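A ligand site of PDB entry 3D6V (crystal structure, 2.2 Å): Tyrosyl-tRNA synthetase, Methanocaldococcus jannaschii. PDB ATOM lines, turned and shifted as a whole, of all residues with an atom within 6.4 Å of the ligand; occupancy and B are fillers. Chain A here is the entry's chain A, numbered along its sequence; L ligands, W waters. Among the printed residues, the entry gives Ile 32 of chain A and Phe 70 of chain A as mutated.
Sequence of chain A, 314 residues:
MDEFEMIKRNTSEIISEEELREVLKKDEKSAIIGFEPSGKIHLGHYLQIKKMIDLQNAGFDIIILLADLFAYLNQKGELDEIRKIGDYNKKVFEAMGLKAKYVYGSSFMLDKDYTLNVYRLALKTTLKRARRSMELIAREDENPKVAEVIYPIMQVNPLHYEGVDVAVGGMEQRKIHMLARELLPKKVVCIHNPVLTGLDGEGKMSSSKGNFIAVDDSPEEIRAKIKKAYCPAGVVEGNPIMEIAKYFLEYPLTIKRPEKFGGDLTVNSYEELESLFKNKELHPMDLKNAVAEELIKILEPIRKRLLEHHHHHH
A nitrogen (N1) of the ligand is in hydrogen-bond range of the side-chain amide oxygen (OE1) of Gln 173.
The side-chain hydroxyl (OH) of Tyr 151 sits at hydrogen-bond distance from a nitrogen (N1) of the ligand (2.8 Å).
N1 of the ligand sits at hydrogen-bond distance from OE1 of Gln 155, 2.9 Å away.
The backbone NH (N) of Glu 36 is in hydrogen-bond range of an oxygen (O1) of the ligand.
CD1 of Ile 32 touches F2 of the ligand (3.5 Å).
Gly 34 touches the ligand.
Phe 35 touches the ligand (CA to O1, 3.9 Å).
Leu 65 touches the ligand.
Ala 67 touches the ligand (CB to C5, 3.7 Å).
Phe 70 touches the ligand (CE2 to C4, 3.6 Å).
CB of His 160 touches F2 of the ligand, 3.5 Å away.
OH of Tyr 161 touches C2 of the ligand (3.2 Å).
Hydrophobic or aromatic side chains that line the ligand: Ile 32, Leu 65, Ala 67, Phe 70, Tyr 151, His 160 and Tyr 161.
Within 4 Å of the ligand: Ile 32, Gly 34, Phe 35, Glu 36, Leu 65, Ala 67, Phe 70, Tyr 151, Gln 155, His 160, Tyr 161 and Gln 173.
Along chain A the residues within 4 Å of the ligand span positions 32 to 173.
NE2 of Gln 173 is in hydrogen-bond range of OE2 of Glu 172, at 3.0 Å.
The side-chain hydroxyl of Tyr 151 is in hydrogen-bond range of the side-chain carboxylate of Glu 36 (2.4 Å).
The backbone carbonyl oxygen (O) of Leu 65 sits at hydrogen-bond distance from the backbone NH (N) of Phe 35 (3.0 Å).
The backbone NH (N) of Leu 65 lies within hydrogen-bond range of the backbone carbonyl oxygen (O) of Ile 33, 3.0 Å away.
The side-chain hydroxyl (OH) of Tyr 161 sits at hydrogen-bond distance from the backbone carbonyl oxygen (O) of Gln 155, at 2.8 Å.
The side-chain carboxylate (OE2) of Glu 36 sits close to the side-chain amide oxygen (OD1) of Asn 74.
The backbone NH (N) of Val 168 is in hydrogen-bond range of the backbone carbonyl oxygen (O) of Ile 32.
The backbone NH (N) of Ala 67 sits at hydrogen-bond distance from the backbone carbonyl oxygen (O) of Phe 35.
Water W1 bridges O2 of the ligand and OE2 of Glu 36.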
ATOM      1  N   ILE A  32       6.787 -31.621 -35.947  1.00  0.00           N
ATOM      2  CA  ILE A  32       6.443 -30.218 -36.004  1.00  0.00           C
ATOM      3  C   ILE A  32       7.520 -29.344 -35.316  1.00  0.00           C
ATOM      4  O   ILE A  32       8.154 -29.788 -34.376  1.00  0.00           O
ATOM      5  CB  ILE A  32       5.008 -29.995 -35.365  1.00  0.00           C
ATOM      6  CG1 ILE A  32       4.392 -28.638 -35.730  1.00  0.00           C
ATOM      7  CG2 ILE A  32       5.083 -30.128 -33.774  1.00  0.00           C
ATOM      8  CD1 ILE A  32       2.831 -28.626 -35.607  1.00  0.00           C
ATOM      9  N   ILE A  33       7.701 -28.103 -35.796  1.00  0.00           N
ATOM     10  CA  ILE A  33       8.468 -27.095 -35.085  1.00  0.00           C
ATOM     11  C   ILE A  33       7.715 -25.792 -35.231  1.00  0.00           C
ATOM     12  O   ILE A  33       7.109 -25.600 -36.263  1.00  0.00           O
ATOM     13  CB  ILE A  33       9.955 -26.908 -35.604  1.00  0.00           C
ATOM     14  CG1 ILE A  33      10.693 -25.788 -34.757  1.00  0.00           C
ATOM     15  CG2 ILE A  33       9.993 -26.582 -37.065  1.00  0.00           C
ATOM     16  CD1 ILE A  33      12.352 -25.953 -34.798  1.00  0.00           C
ATOM     17  N   GLY A  34       7.645 -24.935 -34.160  1.00  0.00           N
ATOM     18  CA  GLY A  34       7.031 -23.582 -34.375  1.00  0.00           C
ATOM     19  C   GLY A  34       8.062 -22.496 -34.276  1.00  0.00           C
ATOM     20  O   GLY A  34       8.948 -22.582 -33.446  1.00  0.00           O
ATOM     21  N   PHE A  35       7.909 -21.417 -35.052  1.00  0.00           N
ATOM     22  CA  PHE A  35       8.785 -20.222 -34.876  1.00  0.00           C
ATOM     23  C   PHE A  35       7.992 -18.927 -34.795  1.00  0.00           C
ATOM     24  O   PHE A  35       7.165 -18.741 -35.647  1.00  0.00           O
ATOM     25  CB  PHE A  35       9.635 -20.017 -36.121  1.00  0.00           C
ATOM     26  CG  PHE A  35      10.699 -20.999 -36.306  1.00  0.00           C
ATOM     27  CD1 PHE A  35      10.532 -22.024 -37.226  1.00  0.00           C
ATOM     28  CD2 PHE A  35      11.886 -20.897 -35.571  1.00  0.00           C
ATOM     29  CE1 PHE A  35      11.593 -22.949 -37.476  1.00  0.00           C
ATOM     30  CE2 PHE A  35      12.919 -21.860 -35.738  1.00  0.00           C
ATOM     31  CZ  PHE A  35      12.766 -22.881 -36.705  1.00  0.00           C
ATOM     32  N   GLU A  36       8.226 -18.065 -33.803  1.00  0.00           N
ATOM     33  CA  GLU A  36       7.763 -16.664 -33.944  1.00  0.00           C
ATOM     34  C   GLU A  36       8.445 -16.014 -35.168  1.00  0.00           C
ATOM     35  O   GLU A  36       9.679 -16.061 -35.268  1.00  0.00           O
ATOM     36  CB  GLU A  36       8.025 -15.804 -32.670  1.00  0.00           C
ATOM     37  CG  GLU A  36       7.291 -16.268 -31.392  1.00  0.00           C
ATOM     38  CD  GLU A  36       7.761 -15.381 -30.177  1.00  0.00           C
ATOM     39  OE1 GLU A  36       7.976 -14.178 -30.414  1.00  0.00           O
ATOM     40  OE2 GLU A  36       7.950 -15.857 -29.031  1.00  0.00           O
ATOM     41  N   LEU A  65       5.116 -24.396 -38.130  1.00  0.00           N
ATOM     42  CA  LEU A  65       4.070 -23.521 -37.683  1.00  0.00           C
ATOM     43  C   LEU A  65       4.666 -22.105 -37.660  1.00  0.00           C
ATOM     44  O   LEU A  65       5.618 -21.824 -36.906  1.00  0.00           O
ATOM     45  CB  LEU A  65       3.575 -23.939 -36.287  1.00  0.00           C
ATOM     46  CG  LEU A  65       2.683 -22.857 -35.619  1.00  0.00           C
ATOM     47  CD1 LEU A  65       1.294 -22.895 -36.320  1.00  0.00           C
ATOM     48  CD2 LEU A  65       2.524 -23.139 -34.179  1.00  0.00           C
ATOM     49  N   ALA A  67       4.351 -19.006 -36.177  1.00  0.00           N
ATOM     50  CA  ALA A  67       3.524 -18.885 -34.929  1.00  0.00           C
ATOM     51  C   ALA A  67       3.236 -17.387 -34.766  1.00  0.00           C
ATOM     52  O   ALA A  67       3.771 -16.752 -33.858  1.00  0.00           O
ATOM     53  CB  ALA A  67       4.317 -19.454 -33.753  1.00  0.00           C
ATOM     54  N   PHE A  70       1.484 -16.029 -31.502  1.00  0.00           N
ATOM     55  CA  PHE A  70       2.480 -16.166 -30.437  1.00  0.00           C
ATOM     56  C   PHE A  70       3.394 -14.940 -30.447  1.00  0.00           C
ATOM     57  O   PHE A  70       3.693 -14.406 -29.396  1.00  0.00           O
ATOM     58  CB  PHE A  70       3.287 -17.494 -30.546  1.00  0.00           C
ATOM     59  CG  PHE A  70       2.508 -18.774 -30.122  1.00  0.00           C
ATOM     60  CD1 PHE A  70       2.505 -19.218 -28.809  1.00  0.00           C
ATOM     61  CD2 PHE A  70       1.811 -19.542 -31.067  1.00  0.00           C
ATOM     62  CE1 PHE A  70       1.824 -20.416 -28.414  1.00  0.00           C
ATOM     63  CE2 PHE A  70       1.099 -20.742 -30.694  1.00  0.00           C
ATOM     64  CZ  PHE A  70       1.101 -21.200 -29.398  1.00  0.00           C
ATOM     65  N   ASN A  74       3.865 -12.069 -27.670  1.00  0.00           N
ATOM     66  CA  ASN A  74       5.179 -11.695 -27.201  1.00  0.00           C
ATOM     67  C   ASN A  74       5.581 -10.274 -27.698  1.00  0.00           C
ATOM     68  O   ASN A  74       6.746  -9.957 -27.766  1.00  0.00           O
ATOM     69  CB  ASN A  74       6.187 -12.743 -27.596  1.00  0.00           C
ATOM     70  CG  ASN A  74       7.212 -13.041 -26.521  1.00  0.00           C
ATOM     71  OD1 ASN A  74       8.165 -13.800 -26.778  1.00  0.00           O
ATOM     72  ND2 ASN A  74       7.093 -12.442 -25.361  1.00  0.00           N
ATOM     73  N   ILE A 137      11.973 -16.946 -22.654  1.00  0.00           N
ATOM     74  CA  ILE A 137      11.209 -16.629 -23.904  1.00  0.00           C
ATOM     75  C   ILE A 137      10.610 -15.201 -23.926  1.00  0.00           C
ATOM     76  O   ILE A 137      10.573 -14.542 -24.960  1.00  0.00           O
ATOM     77  CB  ILE A 137      10.057 -17.731 -24.046  1.00  0.00           C
ATOM     78  CG1 ILE A 137      10.710 -19.094 -24.213  1.00  0.00           C
ATOM     79  CG2 ILE A 137       9.046 -17.407 -25.110  1.00  0.00           C
ATOM     80  CD1 ILE A 137       9.866 -20.216 -23.763  1.00  0.00           C
ATOM     81  N   TYR A 151       0.658 -17.169 -23.401  1.00  0.00           N
ATOM     82  CA  TYR A 151       1.528 -17.768 -24.393  1.00  0.00           C
ATOM     83  C   TYR A 151       1.812 -19.238 -24.124  1.00  0.00           C
ATOM     84  O   TYR A 151       1.674 -20.038 -25.022  1.00  0.00           O
ATOM     85  CB  TYR A 151       2.769 -16.952 -24.460  1.00  0.00           C
ATOM     86  CG  TYR A 151       3.783 -17.232 -25.466  1.00  0.00           C
ATOM     87  CD1 TYR A 151       4.081 -16.283 -26.467  1.00  0.00           C
ATOM     88  CD2 TYR A 151       4.542 -18.373 -25.417  1.00  0.00           C
ATOM     89  CE1 TYR A 151       5.103 -16.531 -27.451  1.00  0.00           C
ATOM     90  CE2 TYR A 151       5.565 -18.643 -26.441  1.00  0.00           C
ATOM     91  CZ  TYR A 151       5.871 -17.698 -27.384  1.00  0.00           C
ATOM     92  OH  TYR A 151       6.905 -17.933 -28.300  1.00  0.00           O
ATOM     93  N   MET A 154      -1.140 -21.590 -24.666  1.00  0.00           N
ATOM     94  CA  MET A 154      -1.465 -21.850 -26.059  1.00  0.00           C
ATOM     95  C   MET A 154      -0.438 -22.823 -26.665  1.00  0.00           C
ATOM     96  O   MET A 154      -0.827 -23.734 -27.326  1.00  0.00           O
ATOM     97  CB  MET A 154      -1.468 -20.555 -26.864  1.00  0.00           C
ATOM     98  CG  MET A 154      -2.662 -19.646 -26.522  1.00  0.00           C
ATOM     99  SD  MET A 154      -2.330 -18.228 -27.537  1.00  0.00           S
ATOM    100  CE  MET A 154      -4.017 -18.024 -28.126  1.00  0.00           C
ATOM    101  N   GLN A 155       0.884 -22.614 -26.428  1.00  0.00           N
ATOM    102  CA  GLN A 155       1.899 -23.594 -26.872  1.00  0.00           C
ATOM    103  C   GLN A 155       1.627 -25.095 -26.521  1.00  0.00           C
ATOM    104  O   GLN A 155       2.086 -25.966 -27.274  1.00  0.00           O
ATOM    105  CB  GLN A 155       3.318 -23.203 -26.429  1.00  0.00           C
ATOM    106  CG  GLN A 155       4.451 -24.024 -27.060  1.00  0.00           C
ATOM    107  CD  GLN A 155       5.715 -23.304 -27.067  1.00  0.00           C
ATOM    108  OE1 GLN A 155       5.733 -22.093 -27.171  1.00  0.00           O
ATOM    109  NE2 GLN A 155       6.795 -24.018 -27.017  1.00  0.00           N
ATOM    110  N   VAL A 156       0.954 -25.403 -25.405  1.00  0.00           N
ATOM    111  CA  VAL A 156       0.665 -26.784 -25.080  1.00  0.00           C
ATOM    112  C   VAL A 156      -0.784 -27.249 -25.438  1.00  0.00           C
ATOM    113  O   VAL A 156      -1.233 -28.262 -24.963  1.00  0.00           O
ATOM    114  CB  VAL A 156       0.968 -27.077 -23.608  1.00  0.00           C
ATOM    115  CG1 VAL A 156       2.436 -26.650 -23.272  1.00  0.00           C
ATOM    116  CG2 VAL A 156      -0.049 -26.451 -22.675  1.00  0.00           C
ATOM    117  N   HIS A 160      -2.422 -28.412 -31.527  1.00  0.00           N
ATOM    118  CA  HIS A 160      -1.204 -28.208 -32.229  1.00  0.00           C
ATOM    119  C   HIS A 160      -0.564 -29.511 -32.571  1.00  0.00           C
ATOM    120  O   HIS A 160       0.261 -29.521 -33.434  1.00  0.00           O
ATOM    121  CB  HIS A 160      -0.208 -27.422 -31.380  1.00  0.00           C
ATOM    122  CG  HIS A 160      -0.471 -25.956 -31.361  1.00  0.00           C
ATOM    123  ND1 HIS A 160      -0.542 -25.184 -32.495  1.00  0.00           N
ATOM    124  CD2 HIS A 160      -0.719 -25.111 -30.337  1.00  0.00           C
ATOM    125  CE1 HIS A 160      -0.787 -23.928 -32.170  1.00  0.00           C
ATOM    126  NE2 HIS A 160      -0.916 -23.870 -30.862  1.00  0.00           N
ATOM    127  N   TYR A 161      -0.933 -30.583 -31.853  1.00  0.00           N
ATOM    128  CA  TYR A 161      -0.245 -31.873 -31.850  1.00  0.00           C
ATOM    129  C   TYR A 161      -1.062 -33.026 -32.365  1.00  0.00           C
ATOM    130  O   TYR A 161      -0.590 -34.158 -32.244  1.00  0.00           O
ATOM    131  CB  TYR A 161       0.342 -32.250 -30.465  1.00  0.00           C
ATOM    132  CG  TYR A 161       1.234 -31.117 -29.947  1.00  0.00           C
ATOM    133  CD1 TYR A 161       2.584 -31.000 -30.367  1.00  0.00           C
ATOM    134  CD2 TYR A 161       0.697 -30.114 -29.126  1.00  0.00           C
ATOM    135  CE1 TYR A 161       3.365 -29.934 -29.930  1.00  0.00           C
ATOM    136  CE2 TYR A 161       1.484 -29.023 -28.672  1.00  0.00           C
ATOM    137  CZ  TYR A 161       2.793 -28.963 -29.067  1.00  0.00           C
ATOM    138  OH  TYR A 161       3.544 -27.929 -28.662  1.00  0.00           O
ATOM    139  N   ALA A 167       7.885 -33.237 -31.619  1.00  0.00           N
ATOM    140  CA  ALA A 167       7.983 -31.800 -31.685  1.00  0.00           C
ATOM    141  C   ALA A 167       9.444 -31.519 -31.496  1.00  0.00           C
ATOM    142  O   ALA A 167      10.087 -32.163 -30.683  1.00  0.00           O
ATOM    143  CB  ALA A 167       7.161 -31.138 -30.494  1.00  0.00           C
ATOM    144  N   VAL A 168       9.972 -30.515 -32.205  1.00  0.00           N
ATOM    145  CA  VAL A 168      11.425 -30.157 -32.127  1.00  0.00           C
ATOM    146  C   VAL A 168      11.448 -28.690 -31.683  1.00  0.00           C
ATOM    147  O   VAL A 168      10.602 -27.894 -32.101  1.00  0.00           O
ATOM    148  CB  VAL A 168      12.123 -30.320 -33.502  1.00  0.00           C
ATOM    149  CG1 VAL A 168      13.632 -29.834 -33.504  1.00  0.00           C
ATOM    150  CG2 VAL A 168      11.943 -31.860 -34.054  1.00  0.00           C
ATOM    151  N   GLU A 172      15.712 -23.580 -24.671  1.00  0.00           N
ATOM    152  CA  GLU A 172      15.019 -22.480 -24.010  1.00  0.00           C
ATOM    153  C   GLU A 172      13.510 -22.749 -23.926  1.00  0.00           C
ATOM    154  O   GLU A 172      12.836 -22.166 -23.072  1.00  0.00           O
ATOM    155  CB  GLU A 172      15.408 -21.074 -24.627  1.00  0.00           C
ATOM    156  CG  GLU A 172      14.713 -20.604 -25.965  1.00  0.00           C
ATOM    157  CD  GLU A 172      15.038 -21.496 -27.256  1.00  0.00           C
ATOM    158  OE1 GLU A 172      16.094 -22.218 -27.205  1.00  0.00           O
ATOM    159  OE2 GLU A 172      14.223 -21.488 -28.306  1.00  0.00           O
ATOM    160  N   GLN A 173      12.962 -23.676 -24.745  1.00  0.00           N
ATOM    161  CA  GLN A 173      11.535 -24.097 -24.648  1.00  0.00           C
ATOM    162  C   GLN A 173      11.286 -25.276 -23.671  1.00  0.00           C
ATOM    163  O   GLN A 173      10.205 -25.760 -23.642  1.00  0.00           O
ATOM    164  CB  GLN A 173      11.028 -24.657 -25.969  1.00  0.00           C
ATOM    165  CG  GLN A 173      11.325 -23.876 -27.231  1.00  0.00           C
ATOM    166  CD  GLN A 173      10.600 -22.584 -27.279  1.00  0.00           C
ATOM    167  OE1 GLN A 173       9.364 -22.552 -27.138  1.00  0.00           O
ATOM    168  NE2 GLN A 173      11.353 -21.479 -27.455  1.00  0.00           N
ATOM    169  N   ILE A 176       8.312 -25.117 -21.018  1.00  0.00           N
ATOM    170  CA  ILE A 176       7.011 -25.194 -21.640  1.00  0.00           C
ATOM    171  C   ILE A 176       6.714 -26.651 -22.110  1.00  0.00           C
ATOM    172  O   ILE A 176       5.593 -27.101 -21.971  1.00  0.00           O
ATOM    173  CB  ILE A 176       6.909 -24.322 -22.858  1.00  0.00           C
ATOM    174  CG1 ILE A 176       6.920 -22.808 -22.478  1.00  0.00           C
ATOM    175  CG2 ILE A 176       5.532 -24.600 -23.518  1.00  0.00           C
ATOM    176  CD1 ILE A 176       7.077 -21.920 -23.629  1.00  0.00           C
ATOM    177  N   HIS A 177       7.695 -27.348 -22.705  1.00  0.00           N
ATOM    178  CA  HIS A 177       7.488 -28.768 -23.098  1.00  0.00           C
ATOM    179  C   HIS A 177       7.286 -29.685 -21.980  1.00  0.00           C
ATOM    180  O   HIS A 177       6.489 -30.596 -22.150  1.00  0.00           O
ATOM    181  CB  HIS A 177       8.641 -29.283 -23.934  1.00  0.00           C
ATOM    182  CG  HIS A 177       8.696 -28.578 -25.233  1.00  0.00           C
ATOM    183  ND1 HIS A 177       9.806 -28.551 -26.036  1.00  0.00           N
ATOM    184  CD2 HIS A 177       7.747 -27.834 -25.848  1.00  0.00           C
ATOM    185  CE1 HIS A 177       9.532 -27.848 -27.122  1.00  0.00           C
ATOM    186  NE2 HIS A 177       8.299 -27.379 -27.011  1.00  0.00           N
HETATM  187  F1  LIG L   1       3.768 -25.398 -33.068  1.00  0.00           F
HETATM  188  C1  LIG L   1       3.925 -26.250 -32.101  1.00  0.00           C
HETATM  189  F2  LIG L   1       3.142 -27.278 -32.395  1.00  0.00           F
HETATM  190  F3  LIG L   1       5.177 -26.712 -32.122  1.00  0.00           F
HETATM  191  C2  LIG L   1       3.565 -25.487 -30.788  1.00  0.00           C
HETATM  192  C3  LIG L   1       4.430 -24.254 -30.809  1.00  0.00           C
HETATM  193  C4  LIG L   1       3.911 -22.973 -30.915  1.00  0.00           C
HETATM  194  C5  LIG L   1       4.804 -21.843 -30.922  1.00  0.00           C
HETATM  195  C6  LIG L   1       5.831 -24.356 -30.688  1.00  0.00           C
HETATM  196  C7  LIG L   1       6.699 -23.241 -30.682  1.00  0.00           C
HETATM  197  C8  LIG L   1       6.185 -21.943 -30.777  1.00  0.00           C
HETATM  198  C9  LIG L   1       7.150 -20.716 -30.790  1.00  0.00           C
HETATM  199  C10 LIG L   1       8.272 -20.777 -29.736  1.00  0.00           C
HETATM  200  N1  LIG L   1       7.882 -20.539 -28.309  1.00  0.00           N
HETATM  201  C11 LIG L   1       9.265 -19.694 -29.982  1.00  0.00           C
HETATM  202  O1  LIG L   1       9.424 -19.281 -31.143  1.00  0.00           O
HETATM  203  O2  LIG L   1       9.849 -19.241 -28.950  1.00  0.00           O
HETATM  204  O   HOH W   1      11.022 -16.809 -28.961  1.00  0.00           O
